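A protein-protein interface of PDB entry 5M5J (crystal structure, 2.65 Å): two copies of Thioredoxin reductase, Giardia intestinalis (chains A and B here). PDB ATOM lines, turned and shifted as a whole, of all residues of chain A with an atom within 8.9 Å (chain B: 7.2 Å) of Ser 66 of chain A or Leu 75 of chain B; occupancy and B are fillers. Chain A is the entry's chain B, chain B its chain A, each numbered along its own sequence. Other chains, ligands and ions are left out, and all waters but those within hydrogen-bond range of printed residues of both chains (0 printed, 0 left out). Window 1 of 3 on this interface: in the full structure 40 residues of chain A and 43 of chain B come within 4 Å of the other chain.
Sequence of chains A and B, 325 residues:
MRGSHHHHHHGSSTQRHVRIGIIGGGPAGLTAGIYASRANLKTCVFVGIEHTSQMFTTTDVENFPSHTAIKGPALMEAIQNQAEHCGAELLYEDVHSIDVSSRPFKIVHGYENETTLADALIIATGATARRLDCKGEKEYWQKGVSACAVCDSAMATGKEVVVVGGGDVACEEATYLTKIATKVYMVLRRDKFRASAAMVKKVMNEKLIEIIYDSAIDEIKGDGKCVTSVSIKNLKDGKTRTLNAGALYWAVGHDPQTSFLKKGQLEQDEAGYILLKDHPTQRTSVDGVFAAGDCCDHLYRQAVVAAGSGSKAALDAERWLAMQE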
ATOM      1  N   VAL A  61     -22.602  -7.738  15.977  1.00  0.00           N
ATOM      2  CA  VAL A  61     -22.189  -8.549  14.828  1.00  0.00           C
ATOM      3  C   VAL A  61     -23.416  -9.295  14.335  1.00  0.00           C
ATOM      4  O   VAL A  61     -24.005 -10.097  15.081  1.00  0.00           O
ATOM      5  CB  VAL A  61     -21.082  -9.570  15.192  1.00  0.00           C
ATOM      6  CG1 VAL A  61     -20.690 -10.399  13.973  1.00  0.00           C
ATOM      7  CG2 VAL A  61     -19.869  -8.865  15.774  1.00  0.00           C
ATOM      8  N   GLU A  62     -23.794  -9.018  13.089  1.00  0.00           N
ATOM      9  CA  GLU A  62     -25.020  -9.554  12.501  1.00  0.00           C
ATOM     10  C   GLU A  62     -24.779 -10.452  11.286  1.00  0.00           C
ATOM     11  O   GLU A  62     -25.712 -11.090  10.800  1.00  0.00           O
ATOM     12  CB  GLU A  62     -25.945  -8.392  12.123  1.00  0.00           C
ATOM     13  CG  GLU A  62     -26.093  -7.334  13.219  1.00  0.00           C
ATOM     14  CD  GLU A  62     -27.432  -6.604  13.202  1.00  0.00           C
ATOM     15  OE1 GLU A  62     -27.819  -6.069  12.137  1.00  0.00           O
ATOM     16  OE2 GLU A  62     -28.087  -6.553  14.268  1.00  0.00           O
ATOM     17  N   ASN A  63     -23.534 -10.528  10.821  1.00  0.00           N
ATOM     18  CA  ASN A  63     -23.209 -11.212   9.580  1.00  0.00           C
ATOM     19  C   ASN A  63     -22.211 -12.378   9.760  1.00  0.00           C
ATOM     20  O   ASN A  63     -21.509 -12.743   8.808  1.00  0.00           O
ATOM     21  CB  ASN A  63     -22.696 -10.188   8.563  1.00  0.00           C
ATOM     22  CG  ASN A  63     -21.457  -9.459   9.040  1.00  0.00           C
ATOM     23  OD1 ASN A  63     -21.047  -9.594  10.194  1.00  0.00           O
ATOM     24  ND2 ASN A  63     -20.855  -8.681   8.156  1.00  0.00           N
ATOM     25  N   PHE A  64     -22.140 -12.940  10.976  1.00  0.00           N
ATOM     26  CA  PHE A  64     -21.384 -14.159  11.228  1.00  0.00           C
ATOM     27  C   PHE A  64     -22.342 -15.351  11.198  1.00  0.00           C
ATOM     28  O   PHE A  64     -23.310 -15.406  11.984  1.00  0.00           O
ATOM     29  CB  PHE A  64     -20.637 -14.116  12.560  1.00  0.00           C
ATOM     30  CG  PHE A  64     -19.494 -15.100  12.635  1.00  0.00           C
ATOM     31  CD1 PHE A  64     -18.254 -14.780  12.097  1.00  0.00           C
ATOM     32  CD2 PHE A  64     -19.655 -16.345  13.220  1.00  0.00           C
ATOM     33  CE1 PHE A  64     -17.196 -15.679  12.153  1.00  0.00           C
ATOM     34  CE2 PHE A  64     -18.599 -17.250  13.272  1.00  0.00           C
ATOM     35  CZ  PHE A  64     -17.368 -16.918  12.737  1.00  0.00           C
ATOM     36  N   PRO A  65     -22.090 -16.306  10.291  1.00  0.00           N
ATOM     37  CA  PRO A  65     -23.031 -17.395  10.062  1.00  0.00           C
ATOM     38  C   PRO A  65     -23.362 -18.160  11.343  1.00  0.00           C
ATOM     39  O   PRO A  65     -22.454 -18.495  12.087  1.00  0.00           O
ATOM     40  CB  PRO A  65     -22.300 -18.289   9.050  1.00  0.00           C
ATOM     41  CG  PRO A  65     -20.873 -17.867   9.084  1.00  0.00           C
ATOM     42  CD  PRO A  65     -20.887 -16.427   9.450  1.00  0.00           C
ATOM     43  N   SER A  66     -24.663 -18.392  11.574  1.00  0.00           N
ATOM     44  CA  SER A  66     -25.250 -19.091  12.747  1.00  0.00           C
ATOM     45  C   SER A  66     -25.647 -18.186  13.921  1.00  0.00           C
ATOM     46  O   SER A  66     -26.133 -18.679  14.938  1.00  0.00           O
ATOM     47  CB  SER A  66     -24.364 -20.231  13.263  1.00  0.00           C
ATOM     48  OG  SER A  66     -23.355 -19.758  14.149  1.00  0.00           O
ATOM     49  N   HIS A  67     -25.432 -16.881  13.793  1.00  0.00           N
ATOM     50  CA  HIS A  67     -25.823 -15.933  14.829  1.00  0.00           C
ATOM     51  C   HIS A  67     -26.609 -14.804  14.175  1.00  0.00           C
ATOM     52  O   HIS A  67     -26.066 -14.072  13.348  1.00  0.00           O
ATOM     53  CB  HIS A  67     -24.591 -15.378  15.549  1.00  0.00           C
ATOM     54  CG  HIS A  67     -23.753 -16.429  16.218  1.00  0.00           C
ATOM     55  ND1 HIS A  67     -24.217 -17.208  17.260  1.00  0.00           N
ATOM     56  CD2 HIS A  67     -22.475 -16.824  15.994  1.00  0.00           C
ATOM     57  CE1 HIS A  67     -23.263 -18.039  17.643  1.00  0.00           C
ATOM     58  NE2 HIS A  67     -22.196 -17.824  16.894  1.00  0.00           N
ATOM     59  N   THR A  68     -27.890 -14.681  14.523  1.00  0.00           N
ATOM     60  CA  THR A  68     -28.704 -13.574  14.019  1.00  0.00           C
ATOM     61  C   THR A  68     -28.101 -12.290  14.529  1.00  0.00           C
ATOM     62  O   THR A  68     -27.843 -11.366  13.752  1.00  0.00           O
ATOM     63  CB  THR A  68     -30.166 -13.659  14.469  1.00  0.00           C
ATOM     64  OG1 THR A  68     -30.727 -14.891  14.006  1.00  0.00           O
ATOM     65  CG2 THR A  68     -30.979 -12.488  13.895  1.00  0.00           C
ATOM     66  N   ALA A  69     -27.861 -12.259  15.836  1.00  0.00           N
ATOM     67  CA  ALA A  69     -27.130 -11.168  16.468  1.00  0.00           C
ATOM     68  C   ALA A  69     -26.217 -11.696  17.575  1.00  0.00           C
ATOM     69  O   ALA A  69     -26.607 -12.574  18.354  1.00  0.00           O
ATOM     70  CB  ALA A  69     -28.101 -10.145  17.025  1.00  0.00           C
ATOM     71  N   ILE A  70     -25.000 -11.156  17.629  1.00  0.00           N
ATOM     72  CA  ILE A  70     -24.055 -11.474  18.695  1.00  0.00           C
ATOM     73  C   ILE A  70     -23.085 -10.313  18.919  1.00  0.00           C
ATOM     74  O   ILE A  70     -22.699  -9.621  17.970  1.00  0.00           O
ATOM     75  CB  ILE A  70     -23.291 -12.783  18.391  1.00  0.00           C
ATOM     76  CG1 ILE A  70     -22.566 -13.280  19.648  1.00  0.00           C
ATOM     77  CG2 ILE A  70     -22.333 -12.613  17.215  1.00  0.00           C
ATOM     78  CD1 ILE A  70     -22.219 -14.751  19.601  1.00  0.00           C
ATOM     79  N   LEU A  75     -18.701 -13.305  20.830  1.00  0.00           N
ATOM     80  CA  LEU A  75     -18.291 -14.125  19.697  1.00  0.00           C
ATOM     81  C   LEU A  75     -16.855 -14.570  19.875  1.00  0.00           C
ATOM     82  O   LEU A  75     -16.522 -15.728  19.638  1.00  0.00           O
ATOM     83  CB  LEU A  75     -18.428 -13.364  18.376  1.00  0.00           C
ATOM     84  CG  LEU A  75     -17.994 -14.118  17.114  1.00  0.00           C
ATOM     85  CD1 LEU A  75     -18.939 -15.274  16.825  1.00  0.00           C
ATOM     86  CD2 LEU A  75     -17.904 -13.171  15.925  1.00  0.00           C
ATOM     87  N   VAL A 304     -15.922 -13.853   9.202  1.00  0.00           N
ATOM     88  CA  VAL A 304     -16.121 -15.153   8.556  1.00  0.00           C
ATOM     89  C   VAL A 304     -15.071 -15.405   7.480  1.00  0.00           C
ATOM     90  O   VAL A 304     -14.588 -16.520   7.355  1.00  0.00           O
ATOM     91  CB  VAL A 304     -17.551 -15.324   7.985  1.00  0.00           C
ATOM     92  CG1 VAL A 304     -17.835 -14.356   6.836  1.00  0.00           C
ATOM     93  CG2 VAL A 304     -17.778 -16.756   7.532  1.00  0.00           C
ATOM     94  N   PRO B  27     -23.688 -23.520   3.663  1.00  0.00           N
ATOM     95  CA  PRO B  27     -22.858 -22.485   4.281  1.00  0.00           C
ATOM     96  C   PRO B  27     -22.416 -21.364   3.335  1.00  0.00           C
ATOM     97  O   PRO B  27     -22.444 -20.199   3.725  1.00  0.00           O
ATOM     98  CB  PRO B  27     -21.649 -23.274   4.781  1.00  0.00           C
ATOM     99  CG  PRO B  27     -22.216 -24.604   5.135  1.00  0.00           C
ATOM    100  CD  PRO B  27     -23.265 -24.865   4.087  1.00  0.00           C
ATOM    101  N   LEU B  30     -25.945 -19.633   1.812  1.00  0.00           N
ATOM    102  CA  LEU B  30     -26.643 -18.846   2.840  1.00  0.00           C
ATOM    103  C   LEU B  30     -25.841 -17.640   3.330  1.00  0.00           C
ATOM    104  O   LEU B  30     -26.433 -16.600   3.631  1.00  0.00           O
ATOM    105  CB  LEU B  30     -27.063 -19.725   4.022  1.00  0.00           C
ATOM    106  CG  LEU B  30     -28.097 -20.801   3.677  1.00  0.00           C
ATOM    107  CD1 LEU B  30     -28.342 -21.728   4.859  1.00  0.00           C
ATOM    108  CD2 LEU B  30     -29.403 -20.188   3.188  1.00  0.00           C
ATOM    109  N   THR B  31     -24.514 -17.772   3.412  1.00  0.00           N
ATOM    110  CA  THR B  31     -23.651 -16.659   3.849  1.00  0.00           C
ATOM    111  C   THR B  31     -23.677 -15.539   2.804  1.00  0.00           C
ATOM    112  O   THR B  31     -23.766 -14.363   3.167  1.00  0.00           O
ATOM    113  CB  THR B  31     -22.195 -17.100   4.133  1.00  0.00           C
ATOM    114  OG1 THR B  31     -22.175 -18.033   5.214  1.00  0.00           O
ATOM    115  CG2 THR B  31     -21.321 -15.916   4.535  1.00  0.00           C
ATOM    116  N   ILE B  34     -27.002 -13.714   3.270  1.00  0.00           N
ATOM    117  CA  ILE B  34     -26.843 -12.787   4.408  1.00  0.00           C
ATOM    118  C   ILE B  34     -26.143 -11.490   3.989  1.00  0.00           C
ATOM    119  O   ILE B  34     -26.673 -10.412   4.223  1.00  0.00           O
ATOM    120  CB  ILE B  34     -26.088 -13.464   5.580  1.00  0.00           C
ATOM    121  CG1 ILE B  34     -26.995 -14.510   6.245  1.00  0.00           C
ATOM    122  CG2 ILE B  34     -25.611 -12.452   6.618  1.00  0.00           C
ATOM    123  CD1 ILE B  34     -26.264 -15.601   6.994  1.00  0.00           C
ATOM    124  N   MET B  55     -24.059 -30.723   5.130  1.00  0.00           N
ATOM    125  CA  MET B  55     -24.060 -30.634   6.596  1.00  0.00           C
ATOM    126  C   MET B  55     -25.192 -31.408   7.267  1.00  0.00           C
ATOM    127  O   MET B  55     -25.070 -31.782   8.434  1.00  0.00           O
ATOM    128  CB  MET B  55     -24.066 -29.169   7.069  1.00  0.00           C
ATOM    129  CG  MET B  55     -22.790 -28.399   6.727  1.00  0.00           C
ATOM    130  SD  MET B  55     -21.270 -29.165   7.329  1.00  0.00           S
ATOM    131  CE  MET B  55     -21.364 -28.707   9.054  1.00  0.00           C
ATOM    132  N   PHE B  56     -26.281 -31.649   6.542  1.00  0.00           N
ATOM    133  CA  PHE B  56     -27.372 -32.485   7.060  1.00  0.00           C
ATOM    134  C   PHE B  56     -27.013 -33.973   7.182  1.00  0.00           C
ATOM    135  O   PHE B  56     -27.644 -34.685   7.958  1.00  0.00           O
ATOM    136  CB  PHE B  56     -28.639 -32.305   6.225  1.00  0.00           C
ATOM    137  CG  PHE B  56     -29.311 -30.972   6.424  1.00  0.00           C
ATOM    138  CD1 PHE B  56     -29.966 -30.676   7.621  1.00  0.00           C
ATOM    139  CD2 PHE B  56     -29.313 -30.016   5.422  1.00  0.00           C
ATOM    140  CE1 PHE B  56     -30.597 -29.450   7.816  1.00  0.00           C
ATOM    141  CE2 PHE B  56     -29.949 -28.793   5.610  1.00  0.00           C
ATOM    142  CZ  PHE B  56     -30.593 -28.511   6.809  1.00  0.00           C
ATOM    143  N   VAL B  61     -20.611 -31.405  14.663  1.00  0.00           N
ATOM    144  CA  VAL B  61     -19.681 -30.442  14.094  1.00  0.00           C
ATOM    145  C   VAL B  61     -18.913 -29.796  15.240  1.00  0.00           C
ATOM    146  O   VAL B  61     -19.507 -29.157  16.117  1.00  0.00           O
ATOM    147  CB  VAL B  61     -20.413 -29.369  13.286  1.00  0.00           C
ATOM    148  CG1 VAL B  61     -19.422 -28.437  12.601  1.00  0.00           C
ATOM    149  CG2 VAL B  61     -21.333 -30.019  12.262  1.00  0.00           C
ATOM    150  N   PHE B  64     -16.507 -25.675  13.489  1.00  0.00           N
ATOM    151  CA  PHE B  64     -17.086 -24.421  13.029  1.00  0.00           C
ATOM    152  C   PHE B  64     -16.871 -23.389  14.137  1.00  0.00           C
ATOM    153  O   PHE B  64     -17.305 -23.620  15.269  1.00  0.00           O
ATOM    154  CB  PHE B  64     -18.578 -24.557  12.713  1.00  0.00           C
ATOM    155  CG  PHE B  64     -19.090 -23.483  11.794  1.00  0.00           C
ATOM    156  CD1 PHE B  64     -19.535 -22.267  12.301  1.00  0.00           C
ATOM    157  CD2 PHE B  64     -19.071 -23.665  10.418  1.00  0.00           C
ATOM    158  CE1 PHE B  64     -19.981 -21.271  11.450  1.00  0.00           C
ATOM    159  CE2 PHE B  64     -19.503 -22.668   9.567  1.00  0.00           C
ATOM    160  CZ  PHE B  64     -19.971 -21.473  10.083  1.00  0.00           C
ATOM    161  N   PRO B  65     -16.200 -22.261  13.828  1.00  0.00           N
ATOM    162  CA  PRO B  65     -15.889 -21.278  14.869  1.00  0.00           C
ATOM    163  C   PRO B  65     -17.125 -20.715  15.606  1.00  0.00           C
ATOM    164  O   PRO B  65     -18.126 -20.390  14.968  1.00  0.00           O
ATOM    165  CB  PRO B  65     -15.161 -20.171  14.101  1.00  0.00           C
ATOM    166  CG  PRO B  65     -15.576 -20.340  12.676  1.00  0.00           C
ATOM    167  CD  PRO B  65     -15.758 -21.807  12.498  1.00  0.00           C
ATOM    168  N   SER B  66     -17.013 -20.631  16.937  1.00  0.00           N
ATOM    169  CA  SER B  66     -18.051 -20.155  17.887  1.00  0.00           C
ATOM    170  C   SER B  66     -18.952 -21.266  18.449  1.00  0.00           C
ATOM    171  O   SER B  66     -19.760 -20.991  19.330  1.00  0.00           O
ATOM    172  CB  SER B  66     -18.910 -19.010  17.328  1.00  0.00           C
ATOM    173  OG  SER B  66     -19.992 -19.508  16.554  1.00  0.00           O
ATOM    174  N   HIS B  67     -18.819 -22.498  17.945  1.00  0.00           N
ATOM    175  CA  HIS B  67     -19.524 -23.663  18.476  1.00  0.00           C
ATOM    176  C   HIS B  67     -18.543 -24.753  18.872  1.00  0.00           C
ATOM    177  O   HIS B  67     -17.905 -25.349  18.030  1.00  0.00           O
ATOM    178  CB  HIS B  67     -20.512 -24.220  17.452  1.00  0.00           C
ATOM    179  CG  HIS B  67     -21.572 -23.245  17.065  1.00  0.00           C
ATOM    180  ND1 HIS B  67     -22.637 -22.944  17.885  1.00  0.00           N
ATOM    181  CD2 HIS B  67     -21.707 -22.462  15.969  1.00  0.00           C
ATOM    182  CE1 HIS B  67     -23.391 -22.031  17.305  1.00  0.00           C
ATOM    183  NE2 HIS B  67     -22.847 -21.715  16.144  1.00  0.00           N
ATOM    184  N   ILE B  70     -21.877 -28.641  17.933  1.00  0.00           N
ATOM    185  CA  ILE B  70     -23.223 -28.400  17.412  1.00  0.00           C
ATOM    186  C   ILE B  70     -23.558 -29.449  16.374  1.00  0.00           C
ATOM    187  O   ILE B  70     -22.684 -29.919  15.656  1.00  0.00           O
ATOM    188  CB  ILE B  70     -23.369 -26.985  16.802  1.00  0.00           C
ATOM    189  CG1 ILE B  70     -24.848 -26.670  16.526  1.00  0.00           C
ATOM    190  CG2 ILE B  70     -22.523 -26.828  15.531  1.00  0.00           C
ATOM    191  CD1 ILE B  70     -25.097 -25.227  16.170  1.00  0.00           C
ATOM    192  N   LYS B  71     -24.837 -29.799  16.294  1.00  0.00           N
ATOM    193  CA  LYS B  71     -25.320 -30.747  15.289  1.00  0.00           C
ATOM    194  C   LYS B  71     -25.417 -30.077  13.923  1.00  0.00           C
ATOM    195  O   LYS B  71     -25.798 -28.913  13.832  1.00  0.00           O
ATOM    196  CB  LYS B  71     -26.690 -31.301  15.681  1.00  0.00           C
ATOM    197  CG  LYS B  71     -26.722 -32.036  17.004  1.00  0.00           C
ATOM    198  CD  LYS B  71     -26.002 -33.368  16.927  1.00  0.00           C
ATOM    199  CE  LYS B  71     -26.092 -34.072  18.272  1.00  0.00           C
ATOM    200  NZ  LYS B  71     -25.199 -35.251  18.383  1.00  0.00           N
ATOM    201  N   GLY B  72     -25.087 -30.818  12.871  1.00  0.00           N
ATOM    202  CA  GLY B  72     -25.087 -30.287  11.504  1.00  0.00           C
ATOM    203  C   GLY B  72     -26.396 -29.635  11.080  1.00  0.00           C
ATOM    204  O   GLY B  72     -26.380 -28.517  10.558  1.00  0.00           O
ATOM    205  N   PRO B  73     -27.534 -30.329  11.294  1.00  0.00           N
ATOM    206  CA  PRO B  73     -28.856 -29.764  11.012  1.00  0.00           C
ATOM    207  C   PRO B  73     -29.143 -28.514  11.803  1.00  0.00           C
ATOM    208  O   PRO B  73     -29.676 -27.555  11.249  1.00  0.00           O
ATOM    209  CB  PRO B  73     -29.826 -30.875  11.439  1.00  0.00           C
ATOM    210  CG  PRO B  73     -29.043 -32.127  11.318  1.00  0.00           C
ATOM    211  CD  PRO B  73     -27.621 -31.760  11.650  1.00  0.00           C
ATOM    212  N   ALA B  74     -28.802 -28.535  13.090  1.00  0.00           N
ATOM    213  CA  ALA B  74     -29.039 -27.393  13.979  1.00  0.00           C
ATOM    214  C   ALA B  74     -28.242 -26.182  13.525  1.00  0.00           C
ATOM    215  O   ALA B  74     -28.756 -25.075  13.509  1.00  0.00           O
ATOM    216  CB  ALA B  74     -28.709 -27.748  15.419  1.00  0.00           C
ATOM    217  N   LEU B  75     -26.996 -26.403  13.127  1.00  0.00           N
ATOM    218  CA  LEU B  75     -26.179 -25.338  12.574  1.00  0.00           C
ATOM    219  C   LEU B  75     -26.850 -24.740  11.355  1.00  0.00           C
ATOM    220  O   LEU B  75     -26.996 -23.539  11.272  1.00  0.00           O
ATOM    221  CB  LEU B  75     -24.781 -25.841  12.196  1.00  0.00           C
ATOM    222  CG  LEU B  75     -23.800 -24.783  11.672  1.00  0.00           C
ATOM    223  CD1 LEU B  75     -23.443 -23.793  12.773  1.00  0.00           C
ATOM    224  CD2 LEU B  75     -22.545 -25.446  11.120  1.00  0.00           C
ATOM    225  N   MET B  76     -27.262 -25.594  10.428  1.00  0.00           N
ATOM    226  CA  MET B  76     -27.899 -25.145   9.199  1.00  0.00           C
ATOM    227  C   MET B  76     -29.196 -24.393   9.451  1.00  0.00           C
ATOM    228  O   MET B  76     -29.445 -23.383   8.793  1.00  0.00           O
ATOM    229  CB  MET B  76     -28.119 -26.313   8.244  1.00  0.00           C
ATOM    230  CG  MET B  76     -26.837 -26.944   7.737  1.00  0.00           C
ATOM    231  SD  MET B  76     -25.843 -25.838   6.721  1.00  0.00           S
ATOM    232  CE  MET B  76     -24.799 -25.012   7.914  1.00  0.00           C
ATOM    233  N   GLU B  77     -29.995 -24.851  10.409  1.00  0.00           N
ATOM    234  CA  GLU B  77     -31.200 -24.126  10.771  1.00  0.00           C
ATOM    235  C   GLU B  77     -30.895 -22.728  11.268  1.00  0.00           C
ATOM    236  O   GLU B  77     -31.557 -21.773  10.857  1.00  0.00           O
ATOM    237  CB  GLU B  77     -32.055 -24.884  11.793  1.00  0.00           C
ATOM    238  CG  GLU B  77     -33.397 -25.283  11.216  1.00  0.00           C
ATOM    239  CD  GLU B  77     -34.307 -24.078  10.979  1.00  0.00           C
ATOM    240  OE1 GLU B  77     -34.970 -23.662  11.957  1.00  0.00           O
ATOM    241  OE2 GLU B  77     -34.366 -23.548   9.833  1.00  0.00           O
ATOM    242  N   ALA B  78     -29.889 -22.602  12.129  1.00  0.00           N
ATOM    243  CA  ALA B  78     -29.458 -21.286  12.612  1.00  0.00           C
ATOM    244  C   ALA B  78     -29.006 -20.334  11.484  1.00  0.00           C
ATOM    245  O   ALA B  78     -29.303 -19.136  11.538  1.00  0.00           O
ATOM    246  CB  ALA B  78     -28.361 -21.434  13.656  1.00  0.00           C
ATOM    247  N   ILE B  79     -28.331 -20.871  10.465  1.00  0.00           N
ATOM    248  CA  ILE B  79     -27.825 -20.056   9.347  1.00  0.00           C
ATOM    249  C   ILE B  79     -28.991 -19.671   8.428  1.00  0.00           C
ATOM    250  O   ILE B  79     -29.044 -18.547   7.931  1.00  0.00           O
ATOM    251  CB  ILE B  79     -26.745 -20.770   8.479  1.00  0.00           C
ATOM    252  CG1 ILE B  79     -25.744 -21.587   9.338  1.00  0.00           C
ATOM    253  CG2 ILE B  79     -26.070 -19.754   7.556  1.00  0.00           C
ATOM    254  CD1 ILE B  79     -24.293 -21.189   9.324  1.00  0.00           C
ATOM    255  N   GLN B  80     -29.900 -20.620   8.191  1.00  0.00           N
ATOM    256  CA  GLN B  80     -31.099 -20.388   7.377  1.00  0.00           C
ATOM    257  C   GLN B  80     -31.969 -19.290   7.970  1.00  0.00           C
ATOM    258  O   GLN B  80     -32.306 -18.327   7.289  1.00  0.00           O
ATOM    259  CB  GLN B  80     -31.918 -21.670   7.238  1.00  0.00           C
ATOM    260  CG  GLN B  80     -31.272 -22.713   6.342  1.00  0.00           C
ATOM    261  CD  GLN B  80     -31.887 -24.101   6.471  1.00  0.00           C
ATOM    262  OE1 GLN B  80     -32.931 -24.288   7.099  1.00  0.00           O
ATOM    263  NE2 GLN B  80     -31.238 -25.086   5.859  1.00  0.00           N
ATOM    264  N   ASN B  81     -32.293 -19.420   9.252  1.00  0.00           N
ATOM    265  CA  ASN B  81     -33.094 -18.399   9.942  1.00  0.00           C
ATOM    266  C   ASN B  81     -32.453 -17.033   9.864  1.00  0.00           C
ATOM    267  O   ASN B  81     -33.153 -16.046   9.675  1.00  0.00           O
ATOM    268  CB  ASN B  81     -33.317 -18.759  11.409  1.00  0.00           C
ATOM    269  CG  ASN B  81     -34.131 -20.022  11.586  1.00  0.00           C
ATOM    270  OD1 ASN B  81     -34.808 -20.487  10.664  1.00  0.00           O
ATOM    271  ND2 ASN B  81     -34.063 -20.593  12.777  1.00  0.00           N
ATOM    272  N   GLN B  82     -31.126 -16.999  10.007  1.00  0.00           N
ATOM    273  CA  GLN B  82     -30.333 -15.772   9.876  1.00  0.00           C
ATOM    274  C   GLN B  82     -30.531 -15.118   8.512  1.00  0.00           C
ATOM    275  O   GLN B  82     -30.887 -13.946   8.441  1.00  0.00           O
ATOM    276  CB  GLN B  82     -28.833 -16.054  10.115  1.00  0.00           C
ATOM    277  CG  GLN B  82     -27.933 -14.816  10.142  1.00  0.00           C
ATOM    278  CD  GLN B  82     -26.489 -15.122  10.510  1.00  0.00           C
ATOM    279  OE1 GLN B  82     -26.145 -16.251  10.881  1.00  0.00           O
ATOM    280  NE2 GLN B  82     -25.632 -14.105  10.417  1.00  0.00           N
ATOM    281  N   ALA B 303     -16.900 -26.250   6.050  1.00  0.00           N
ATOM    282  CA  ALA B 303     -18.049 -25.365   6.137  1.00  0.00           C
ATOM    283  C   ALA B 303     -17.596 -23.917   6.354  1.00  0.00           C
ATOM    284  O   ALA B 303     -18.095 -23.011   5.686  1.00  0.00           O
ATOM    285  CB  ALA B 303     -18.992 -25.815   7.247  1.00  0.00           C
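Asn 63 of chain A touches Gln 82 of chain B. Phe 64 of chain A touches Pro 65 of chain B (CE2 to O, 3.6 Å). Thr 31 of chain B touches Pro 65 of chain A (OG1 to CB, 3.8 Å). Phe 64 of chain B touches Pro 65 of chain A. Pro 65 of chain A touches Ile 79 of chain B (CB to CD1, 3.5 Å). Pro 65 of chain A touches Gln 82 of chain B. Leu 75 of chain B touches Ser 66 of chain A (CD1 to CB, 3.7 Å). Ser 66 of chain A touches Ala 78 of chain B (O to CB, 3.8 Å). N of Ser 66 of chain A touches CD1 of Ile 79 of chain B (3.6 Å). CD1 of Leu 75 of chain A touches CB of Ser 66 of chain B (3.8 Å).
The backbone carbonyl oxygen of Pro 27 of chain B sits at hydrogen-bond distance from the side-chain hydroxyl of Thr 31 of chain B (2.6 Å).
OG of Ser 66 of chain B is in hydrogen-bond range of NE2 of His 67 of chain A. A ring nitrogen (NE2) of His 67 of chain B sits at hydrogen-bond distance from the side-chain hydroxyl of Ser 66 of chain A. NE2 of Gln 82 of chain B lies within hydrogen-bond range of O of Glu 62 of chain A (3.0 Å). NE2 of Gln 82 of chain B lies within hydrogen-bond range of O of Phe 64 of chain A, 3.1 Å away. OE1 of Gln 82 of chain B lies within hydrogen-bond range of N of Ser 66 of chain A. NE2 of Gln 82 of chain B lies within hydrogen-bond range of O of His 67 of chain A (3.0 Å).
Of the 12 printed residues of chain A, 7 touch a printed residue of chain B. Hydrophobic or aromatic side chains of chain A that line the printed part of chain B: Phe 64, Pro 65, His 67 and Leu 75. Of the 25 printed residues of chain B, 9 touch a printed residue of chain A. Printed residues of chain B that touch a printed residue of chain A: Thr 31, Phe 64, Pro 65, Ser 66, His 67, Leu 75, Ala 78, Ile 79 and Gln 82.
Phe 64 of chain A touches Pro 65 of chain B, and with the chains exchanged Pro 65 of chain A touches Phe 64 of chain B. Ser 66 of chain A touches His 67 of chain B, and with the chains exchanged His 67 of chain A touches Ser 66 of chain B. Ser 66 of chain A touches Leu 75 of chain B, and with the chains exchanged Leu 75 of chain A touches Ser 66 of chain B. His 67 of chain B touches its own counterpart, His 67 of chain A. 7 positions are printed for both chains. Of the 17 pairs that touch across the chains among the printed residues, 7 have their exchanged pair printed and touching as well.
Of chain B, only His 67, Leu 75, Ala 78, Ile 79 and Gln 82 come within 4 Å of Ser 66 of chain A. Printed residues of chain B within 4 Å of His 67 of chain A: Ser 66 (2.8 Å), His 67 (3.99 Å) and Gln 82 (3.0 Å). Of the printed residues of chain B, Leu 75 of chain A touches Ser 66. Printed residues of chain A within 4 Å of Phe 64 of chain B: Pro 65 (3.8 Å). Lys 71 of chain B touches none of the printed residues of chain A. Gly 72 of chain B touches none of the printed residues of chain A. No residue of chain A comes within 4 Å of Ala 74 of chain B. Leu 75 of chain B touches just one residue of chain A: Ser 66 (3.7 Å). Ala 78 of chain B touches just one residue of chain A: Ser 66. Printed residues of chain A within 4 Å of Gln 82 of chain B: Glu 62 (3.0 Å), Asn 63 (3.9 Å), Phe 64 (3.1 Å), Pro 65 (3.4 Å), Ser 66 (2.7 Å) and His 67 (3.0 Å). The nearest residue of chain B that does not touch Ser 66 of chain A is Ser 66 of chain B (4.1 Å).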
